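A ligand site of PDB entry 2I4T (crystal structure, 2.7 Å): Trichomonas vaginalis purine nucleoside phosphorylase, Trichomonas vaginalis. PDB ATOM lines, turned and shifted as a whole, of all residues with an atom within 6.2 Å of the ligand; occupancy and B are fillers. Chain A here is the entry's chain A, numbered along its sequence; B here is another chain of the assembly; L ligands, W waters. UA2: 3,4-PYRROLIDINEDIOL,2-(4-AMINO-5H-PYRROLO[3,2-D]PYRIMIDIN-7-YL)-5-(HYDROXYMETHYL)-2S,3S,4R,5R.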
ATOM      1  N   GLY A  20     -18.668  10.096   7.316  1.00  0.00           N
ATOM      2  CA  GLY A  20     -18.759   9.416   8.617  1.00  0.00           C
ATOM      3  C   GLY A  20     -18.844  10.409   9.752  1.00  0.00           C
ATOM      4  O   GLY A  20     -19.665  10.301  10.662  1.00  0.00           O
ATOM      5  N   HIS A  62     -23.052   9.821   8.510  1.00  0.00           N
ATOM      6  CA  HIS A  62     -23.620   8.485   8.741  1.00  0.00           C
ATOM      7  C   HIS A  62     -23.081   7.698   9.939  1.00  0.00           C
ATOM      8  O   HIS A  62     -23.488   6.579  10.146  1.00  0.00           O
ATOM      9  CB  HIS A  62     -23.522   7.607   7.500  1.00  0.00           C
ATOM     10  CG  HIS A  62     -22.166   7.527   6.888  1.00  0.00           C
ATOM     11  ND1 HIS A  62     -21.050   7.066   7.577  1.00  0.00           N
ATOM     12  CD2 HIS A  62     -21.734   7.834   5.632  1.00  0.00           C
ATOM     13  CE1 HIS A  62     -19.986   7.123   6.785  1.00  0.00           C
ATOM     14  NE2 HIS A  62     -20.377   7.585   5.605  1.00  0.00           N
ATOM     15  N   GLY A  63     -22.177   8.244  10.736  1.00  0.00           N
ATOM     16  CA  GLY A  63     -21.505   7.416  11.742  1.00  0.00           C
ATOM     17  C   GLY A  63     -20.517   6.390  11.144  1.00  0.00           C
ATOM     18  O   GLY A  63     -20.374   6.250   9.922  1.00  0.00           O
ATOM     19  N   MET A  64     -19.824   5.650  11.990  1.00  0.00           N
ATOM     20  CA  MET A  64     -18.849   4.694  11.485  1.00  0.00           C
ATOM     21  C   MET A  64     -19.458   3.318  11.450  1.00  0.00           C
ATOM     22  O   MET A  64     -20.057   2.924  12.428  1.00  0.00           O
ATOM     23  CB  MET A  64     -17.633   4.717  12.390  1.00  0.00           C
ATOM     24  CG  MET A  64     -17.067   6.114  12.434  1.00  0.00           C
ATOM     25  SD  MET A  64     -15.370   6.194  13.023  1.00  0.00           S
ATOM     26  CE  MET A  64     -15.707   5.969  14.790  1.00  0.00           C
ATOM     27  N   GLY A  65     -19.360   2.599  10.320  1.00  0.00           N
ATOM     28  CA  GLY A  65     -19.764   1.202  10.263  1.00  0.00           C
ATOM     29  C   GLY A  65     -21.062   0.870   9.555  1.00  0.00           C
ATOM     30  O   GLY A  65     -22.024   1.653   9.546  1.00  0.00           O
ATOM     31  N   ARG A  87     -21.098   8.460  -0.886  1.00  0.00           N
ATOM     32  CA  ARG A  87     -20.245   8.531   0.286  1.00  0.00           C
ATOM     33  C   ARG A  87     -19.020   9.361  -0.064  1.00  0.00           C
ATOM     34  O   ARG A  87     -18.387   9.167  -1.127  1.00  0.00           O
ATOM     35  CB  ARG A  87     -19.813   7.111   0.734  1.00  0.00           C
ATOM     36  CG  ARG A  87     -19.412   6.970   2.219  1.00  0.00           C
ATOM     37  CD  ARG A  87     -18.972   5.560   2.592  1.00  0.00           C
ATOM     38  NE  ARG A  87     -17.553   5.467   2.946  1.00  0.00           N
ATOM     39  CZ  ARG A  87     -17.009   6.231   3.877  1.00  0.00           C
ATOM     40  NH1 ARG A  87     -17.789   7.120   4.488  1.00  0.00           N
ATOM     41  NH2 ARG A  87     -15.706   6.125   4.200  1.00  0.00           N
ATOM     42  N   THR A  90     -12.871   8.787   4.060  1.00  0.00           N
ATOM     43  CA  THR A  90     -11.428   8.516   4.092  1.00  0.00           C
ATOM     44  C   THR A  90     -11.271   7.000   4.137  1.00  0.00           C
ATOM     45  O   THR A  90     -12.212   6.295   4.494  1.00  0.00           O
ATOM     46  CB  THR A  90     -10.805   9.141   5.325  1.00  0.00           C
ATOM     47  OG1 THR A  90     -11.589   8.712   6.449  1.00  0.00           O
ATOM     48  CG2 THR A  90     -10.885  10.636   5.233  1.00  0.00           C
ATOM     49  N   CYS A  91     -10.106   6.488   3.776  1.00  0.00           N
ATOM     50  CA  CYS A  91      -9.888   5.041   3.766  1.00  0.00           C
ATOM     51  C   CYS A  91      -8.427   4.747   4.037  1.00  0.00           C
ATOM     52  O   CYS A  91      -7.613   5.652   3.910  1.00  0.00           O
ATOM     53  CB  CYS A  91     -10.299   4.441   2.424  1.00  0.00           C
ATOM     54  SG  CYS A  91      -9.413   5.182   1.001  1.00  0.00           S
ATOM     55  N   GLY A  92      -8.093   3.520   4.438  1.00  0.00           N
ATOM     56  CA  GLY A  92      -6.687   3.098   4.531  1.00  0.00           C
ATOM     57  C   GLY A  92      -6.273   2.403   3.242  1.00  0.00           C
ATOM     58  O   GLY A  92      -6.957   1.487   2.790  1.00  0.00           O
ATOM     59  N   ALA A  93      -5.176   2.812   2.613  1.00  0.00           N
ATOM     60  CA  ALA A  93      -4.797   2.156   1.351  1.00  0.00           C
ATOM     61  C   ALA A  93      -4.198   0.810   1.609  1.00  0.00           C
ATOM     62  O   ALA A  93      -3.609   0.547   2.700  1.00  0.00           O
ATOM     63  CB  ALA A  93      -3.837   3.003   0.524  1.00  0.00           C
ATOM     64  N   THR A 156     -14.631  -3.151   6.522  1.00  0.00           N
ATOM     65  CA  THR A 156     -14.452  -4.031   7.652  1.00  0.00           C
ATOM     66  C   THR A 156     -15.353  -3.620   8.840  1.00  0.00           C
ATOM     67  O   THR A 156     -15.701  -2.455   9.001  1.00  0.00           O
ATOM     68  CB  THR A 156     -13.004  -3.970   8.132  1.00  0.00           C
ATOM     69  OG1 THR A 156     -12.820  -4.880   9.230  1.00  0.00           O
ATOM     70  CG2 THR A 156     -12.676  -2.570   8.630  1.00  0.00           C
ATOM     71  N   LEU A 158     -14.261  -4.169  11.692  1.00  0.00           N
ATOM     72  CA  LEU A 158     -13.280  -4.181  12.746  1.00  0.00           C
ATOM     73  C   LEU A 158     -12.120  -3.315  12.315  1.00  0.00           C
ATOM     74  O   LEU A 158     -11.341  -3.714  11.424  1.00  0.00           O
ATOM     75  CB  LEU A 158     -12.790  -5.588  12.914  1.00  0.00           C
ATOM     76  CG  LEU A 158     -13.089  -6.387  14.152  1.00  0.00           C
ATOM     77  CD1 LEU A 158     -14.016  -5.696  15.234  1.00  0.00           C
ATOM     78  CD2 LEU A 158     -13.594  -7.745  13.673  1.00  0.00           C
ATOM     79  N   PHE A 159     -12.049  -2.108  12.892  1.00  0.00           N
ATOM     80  CA  PHE A 159     -11.023  -1.141  12.531  1.00  0.00           C
ATOM     81  C   PHE A 159      -9.679  -1.692  13.000  1.00  0.00           C
ATOM     82  O   PHE A 159      -8.722  -1.735  12.235  1.00  0.00           O
ATOM     83  CB  PHE A 159     -11.327   0.245  13.115  1.00  0.00           C
ATOM     84  CG  PHE A 159     -10.260   1.308  12.793  1.00  0.00           C
ATOM     85  CD1 PHE A 159     -10.351   2.080  11.643  1.00  0.00           C
ATOM     86  CD2 PHE A 159      -9.199   1.566  13.694  1.00  0.00           C
ATOM     87  CE1 PHE A 159      -9.373   3.057  11.356  1.00  0.00           C
ATOM     88  CE2 PHE A 159      -8.267   2.571  13.436  1.00  0.00           C
ATOM     89  CZ  PHE A 159      -8.352   3.303  12.256  1.00  0.00           C
ATOM     90  N   VAL A 178      -9.476   0.141   2.308  1.00  0.00           N
ATOM     91  CA  VAL A 178     -10.404  -0.273   3.358  1.00  0.00           C
ATOM     92  C   VAL A 178     -11.130   0.918   3.959  1.00  0.00           C
ATOM     93  O   VAL A 178     -10.498   1.882   4.402  1.00  0.00           O
ATOM     94  CB  VAL A 178      -9.619  -0.922   4.534  1.00  0.00           C
ATOM     95  CG1 VAL A 178     -10.529  -1.295   5.689  1.00  0.00           C
ATOM     96  CG2 VAL A 178      -8.923  -2.158   4.068  1.00  0.00           C
ATOM     97  N   GLU A 179     -12.452   0.864   4.017  1.00  0.00           N
ATOM     98  CA  GLU A 179     -13.181   1.803   4.892  1.00  0.00           C
ATOM     99  C   GLU A 179     -14.200   0.952   5.608  1.00  0.00           C
ATOM    100  O   GLU A 179     -13.974  -0.217   5.758  1.00  0.00           O
ATOM    101  CB  GLU A 179     -13.785   2.952   4.114  1.00  0.00           C
ATOM    102  CG  GLU A 179     -14.300   2.568   2.770  1.00  0.00           C
ATOM    103  CD  GLU A 179     -15.726   2.100   2.811  1.00  0.00           C
ATOM    104  OE1 GLU A 179     -15.912   0.914   3.054  1.00  0.00           O
ATOM    105  OE2 GLU A 179     -16.669   2.906   2.598  1.00  0.00           O
ATOM    106  N   MET A 180     -15.317   1.495   6.070  1.00  0.00           N
ATOM    107  CA  MET A 180     -16.156   0.695   6.971  1.00  0.00           C
ATOM    108  C   MET A 180     -17.659   0.878   6.685  1.00  0.00           C
ATOM    109  O   MET A 180     -18.478   0.722   7.609  1.00  0.00           O
ATOM    110  CB  MET A 180     -15.905   1.084   8.429  1.00  0.00           C
ATOM    111  CG  MET A 180     -14.570   0.778   8.951  1.00  0.00           C
ATOM    112  SD  MET A 180     -14.359   1.443  10.638  1.00  0.00           S
ATOM    113  CE  MET A 180     -15.382   0.300  11.565  1.00  0.00           C
ATOM    114  N   GLU A 181     -18.017   1.240   5.445  1.00  0.00           N
ATOM    115  CA  GLU A 181     -19.429   1.600   5.150  1.00  0.00           C
ATOM    116  C   GLU A 181     -19.961   1.236   3.766  1.00  0.00           C
ATOM    117  O   GLU A 181     -21.121   0.853   3.615  1.00  0.00           O
ATOM    118  CB  GLU A 181     -19.647   3.077   5.434  1.00  0.00           C
ATOM    119  CG  GLU A 181     -19.587   3.419   6.925  1.00  0.00           C
ATOM    120  CD  GLU A 181     -18.231   3.948   7.340  1.00  0.00           C
ATOM    121  OE1 GLU A 181     -17.967   4.025   8.556  1.00  0.00           O
ATOM    122  OE2 GLU A 181     -17.416   4.290   6.445  1.00  0.00           O
ATOM    123  N   THR A 201     -10.587   9.394   0.157  1.00  0.00           N
ATOM    124  CA  THR A 201      -9.287   9.989   0.200  1.00  0.00           C
ATOM    125  C   THR A 201      -8.432   9.117   1.115  1.00  0.00           C
ATOM    126  O   THR A 201      -8.876   8.679   2.177  1.00  0.00           O
ATOM    127  CB  THR A 201      -9.354  11.482   0.666  1.00  0.00           C
ATOM    128  OG1 THR A 201      -8.038  12.034   0.671  1.00  0.00           O
ATOM    129  CG2 THR A 201      -9.895  11.608   2.054  1.00  0.00           C
ATOM    130  N   SER A 203      -6.213   8.311   3.830  1.00  0.00           N
ATOM    131  CA  SER A 203      -5.664   9.040   4.930  1.00  0.00           C
ATOM    132  C   SER A 203      -4.492   8.320   5.618  1.00  0.00           C
ATOM    133  O   SER A 203      -3.999   8.808   6.613  1.00  0.00           O
ATOM    134  CB  SER A 203      -6.759   9.308   5.938  1.00  0.00           C
ATOM    135  OG  SER A 203      -7.151   8.072   6.454  1.00  0.00           O
ATOM    136  N   ASP A 204      -4.069   7.177   5.102  1.00  0.00           N
ATOM    137  CA  ASP A 204      -3.080   6.305   5.791  1.00  0.00           C
ATOM    138  C   ASP A 204      -2.890   5.023   4.974  1.00  0.00           C
ATOM    139  O   ASP A 204      -3.778   4.664   4.208  1.00  0.00           O
ATOM    140  CB  ASP A 204      -3.439   6.042   7.295  1.00  0.00           C
ATOM    141  CG  ASP A 204      -4.703   5.106   7.503  1.00  0.00           C
ATOM    142  OD1 ASP A 204      -4.490   3.880   7.710  1.00  0.00           O
ATOM    143  OD2 ASP A 204      -5.902   5.569   7.528  1.00  0.00           O
ATOM    144  N   HIS A 205      -1.744   4.350   5.088  1.00  0.00           N
ATOM    145  CA  HIS A 205      -1.546   3.101   4.378  1.00  0.00           C
ATOM    146  C   HIS A 205      -1.597   1.922   5.369  1.00  0.00           C
ATOM    147  O   HIS A 205      -0.994   2.004   6.424  1.00  0.00           O
ATOM    148  CB  HIS A 205      -0.230   3.083   3.627  1.00  0.00           C
ATOM    149  CG  HIS A 205      -0.276   2.227   2.405  1.00  0.00           C
ATOM    150  ND1 HIS A 205      -0.119   0.860   2.458  1.00  0.00           N
ATOM    151  CD2 HIS A 205      -0.576   2.524   1.117  1.00  0.00           C
ATOM    152  CE1 HIS A 205      -0.297   0.347   1.245  1.00  0.00           C
ATOM    153  NE2 HIS A 205      -0.574   1.335   0.418  1.00  0.00           N
ATOM    154  N   ILE A 206      -2.309   0.846   5.086  1.00  0.00           N
ATOM    155  CA  ILE A 206      -2.310  -0.216   6.112  1.00  0.00           C
ATOM    156  C   ILE A 206      -1.079  -1.121   5.927  1.00  0.00           C
ATOM    157  O   ILE A 206      -0.638  -1.778   6.834  1.00  0.00           O
ATOM    158  CB  ILE A 206      -3.611  -1.079   6.147  1.00  0.00           C
ATOM    159  CG1 ILE A 206      -3.554  -2.089   4.993  1.00  0.00           C
ATOM    160  CG2 ILE A 206      -4.919  -0.216   6.126  1.00  0.00           C
ATOM    161  CD1 ILE A 206      -4.913  -2.384   4.277  1.00  0.00           C
ATOM    162  N   PRO B   3      -6.703   7.842  16.437  1.00  0.00           N
ATOM    163  CA  PRO B   3      -7.331   8.533  15.278  1.00  0.00           C
ATOM    164  C   PRO B   3      -8.758   9.021  15.551  1.00  0.00           C
ATOM    165  O   PRO B   3      -9.375   9.687  14.694  1.00  0.00           O
ATOM    166  CB  PRO B   3      -7.357   7.446  14.188  1.00  0.00           C
ATOM    167  CG  PRO B   3      -6.305   6.494  14.604  1.00  0.00           C
ATOM    168  CD  PRO B   3      -6.406   6.444  16.128  1.00  0.00           C
ATOM    169  N   HIS B   4      -9.300   8.694  16.716  1.00  0.00           N
ATOM    170  CA  HIS B   4     -10.728   8.942  16.955  1.00  0.00           C
ATOM    171  C   HIS B   4     -10.813   9.660  18.255  1.00  0.00           C
ATOM    172  O   HIS B   4     -11.896   9.913  18.754  1.00  0.00           O
ATOM    173  CB  HIS B   4     -11.535   7.620  17.048  1.00  0.00           C
ATOM    174  CG  HIS B   4     -11.409   6.769  15.824  1.00  0.00           C
ATOM    175  ND1 HIS B   4     -10.571   5.676  15.752  1.00  0.00           N
ATOM    176  CD2 HIS B   4     -11.937   6.917  14.584  1.00  0.00           C
ATOM    177  CE1 HIS B   4     -10.598   5.183  14.519  1.00  0.00           C
ATOM    178  NE2 HIS B   4     -11.413   5.922  13.785  1.00  0.00           N
ATOM    179  N   ARG B  43     -14.942  14.025  15.586  1.00  0.00           N
ATOM    180  CA  ARG B  43     -16.242  13.450  15.149  1.00  0.00           C
ATOM    181  C   ARG B  43     -17.504  13.834  16.039  1.00  0.00           C
ATOM    182  O   ARG B  43     -18.605  13.219  15.942  1.00  0.00           O
ATOM    183  CB  ARG B  43     -16.110  11.949  14.935  1.00  0.00           C
ATOM    184  CG  ARG B  43     -15.170  11.551  13.748  1.00  0.00           C
ATOM    185  CD  ARG B  43     -14.731  10.049  13.780  1.00  0.00           C
ATOM    186  NE  ARG B  43     -13.790   9.787  12.700  1.00  0.00           N
ATOM    187  CZ  ARG B  43     -14.168   9.433  11.479  1.00  0.00           C
ATOM    188  NH1 ARG B  43     -15.445   9.268  11.260  1.00  0.00           N
ATOM    189  NH2 ARG B  43     -13.281   9.221  10.504  1.00  0.00           N
ATOM    190  N   ILE B  71     -14.491   0.357  18.118  1.00  0.00           N
ATOM    191  CA  ILE B  71     -13.413   1.308  17.946  1.00  0.00           C
ATOM    192  C   ILE B  71     -13.260   2.070  19.261  1.00  0.00           C
ATOM    193  O   ILE B  71     -12.169   2.141  19.780  1.00  0.00           O
ATOM    194  CB  ILE B  71     -13.692   2.333  16.824  1.00  0.00           C
ATOM    195  CG1 ILE B  71     -13.534   1.698  15.446  1.00  0.00           C
ATOM    196  CG2 ILE B  71     -12.760   3.545  16.946  1.00  0.00           C
ATOM    197  CD1 ILE B  71     -13.982   2.633  14.246  1.00  0.00           C
HETATM  198  C2  UA2 L   1     -10.408   1.243   8.346  1.00  0.00           C
HETATM  199  C4  UA2 L   1     -10.758   3.463   7.809  1.00  0.00           C
HETATM  200  C5  UA2 L   1      -9.359   3.617   7.626  1.00  0.00           C
HETATM  201  C6  UA2 L   1      -8.508   2.504   7.835  1.00  0.00           C
HETATM  202  O5' UA2 L   1     -11.372   5.501  10.860  1.00  0.00           O
HETATM  203  C5' UA2 L   1     -12.734   5.122  10.914  1.00  0.00           C
HETATM  204  C4' UA2 L   1     -13.607   5.812   9.883  1.00  0.00           C
HETATM  205  N4' UA2 L   1     -12.826   6.186   8.712  1.00  0.00           N
HETATM  206  C3' UA2 L   1     -14.591   4.819   9.344  1.00  0.00           C
HETATM  207  O3' UA2 L   1     -15.823   5.540   9.153  1.00  0.00           O
HETATM  208  C2' UA2 L   1     -13.932   4.292   8.036  1.00  0.00           C
HETATM  209  O2' UA2 L   1     -14.886   4.366   6.977  1.00  0.00           O
HETATM  210  C1' UA2 L   1     -12.778   5.199   7.634  1.00  0.00           C
HETATM  211  C9  UA2 L   1     -11.341   4.715   7.549  1.00  0.00           C
HETATM  212  N3  UA2 L   1     -11.286   2.268   8.160  1.00  0.00           N
HETATM  213  N1  UA2 L   1      -9.067   1.300   8.196  1.00  0.00           N
HETATM  214  C8  UA2 L   1     -10.315   5.630   7.224  1.00  0.00           C
HETATM  215  N7  UA2 L   1      -9.121   4.939   7.276  1.00  0.00           N
HETATM  216  N6  UA2 L   1      -7.159   2.610   7.671  1.00  0.00           N
HETATM  217  O   HOH W   1      -8.905  -1.666   9.434  1.00  0.00           O
HETATM  218  O   HOH W   2      -9.455   7.906  10.193  1.00  0.00           O
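The side-chain carboxylate of Glu 181 sits at hydrogen-bond distance from an oxygen (O2') of the ligand, at 2.6 Å.
A ring nitrogen (NE2) of His 4 of chain B lies within hydrogen-bond range of an oxygen (O5') of the ligand, at 3.0 Å.
The side-chain carboxylate of Asp 204 sits at hydrogen-bond distance from a nitrogen (N6) of the ligand, 3.0 Å away.
The backbone NH (N) of Met 180 is in hydrogen-bond range of an oxygen (O2') of the ligand (3.0 Å).
N7 of the ligand sits close to N of Gly 92.
An oxygen (O2') of the ligand sits at hydrogen-bond distance from the guanidinium group (NH2) of Arg 87, at 3.4 Å.
The side-chain carboxylate of Glu 181 lies within salt-bridge range of the guanidinium group of Arg 87 (3.4 Å).
The side-chain carboxylate (OE1) of Glu 181 lies within hydrogen-bond range of the backbone NH (N) of Gly 65.
The side-chain carboxylate (OD2) of Asp 204 sits at hydrogen-bond distance from the side-chain hydroxyl (OG) of Ser 203 (3.0 Å).
The backbone carbonyl oxygen of Gly 92 sits at hydrogen-bond distance from the backbone NH of Val 178 (2.9 Å).
The backbone carbonyl oxygen (O) of Cys 91 lies within hydrogen-bond range of the backbone NH (N) of Ser 203.
NE of Arg 87 lies within salt-bridge range of OE2 of Glu 179, at 2.7 Å.
The backbone carbonyl oxygen of Glu 179 lies within hydrogen-bond range of the backbone NH of Thr 156, at 3.1 Å.
The backbone NH (N) of Ile 206 is in hydrogen-bond range of the backbone carbonyl oxygen (O) of Ala 93, 2.7 Å away.
Met 64 touches the ligand.
Thr 90 touches the ligand.
C of Cys 91 touches N7 of the ligand (3.3 Å).
Phe 159 touches the ligand.
Val 178 touches the ligand (CG1 to C2, 3.7 Å).
CB of Glu 179 touches O2' of the ligand (3.4 Å).
Ser 203 touches the ligand.
CG2 of Ile 206 touches N6 of the ligand, 3.9 Å away.
Arg 43 of chain B touches the ligand (NH2 to C4', 3.5 Å).
Hydrophobic or aromatic side chains within 4 Å of the ligand: Met 64, Phe 159, Val 178, Met 180, Ile 206 and His 4 of chain B.
Within 4 Å of the ligand: Met 64, Arg 87, Thr 90, Cys 91, Gly 92, Phe 159, Val 178, Glu 179, Met 180, Glu 181, Ser 203, Asp 204, Ile 206, His 4 of chain B and Arg 43 of chain B.
Water W1 lies within hydrogen-bond range of the backbone carbonyl oxygen (O) of Phe 159 (2.8 Å) and a nitrogen (N1) of the ligand (3.2 Å).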
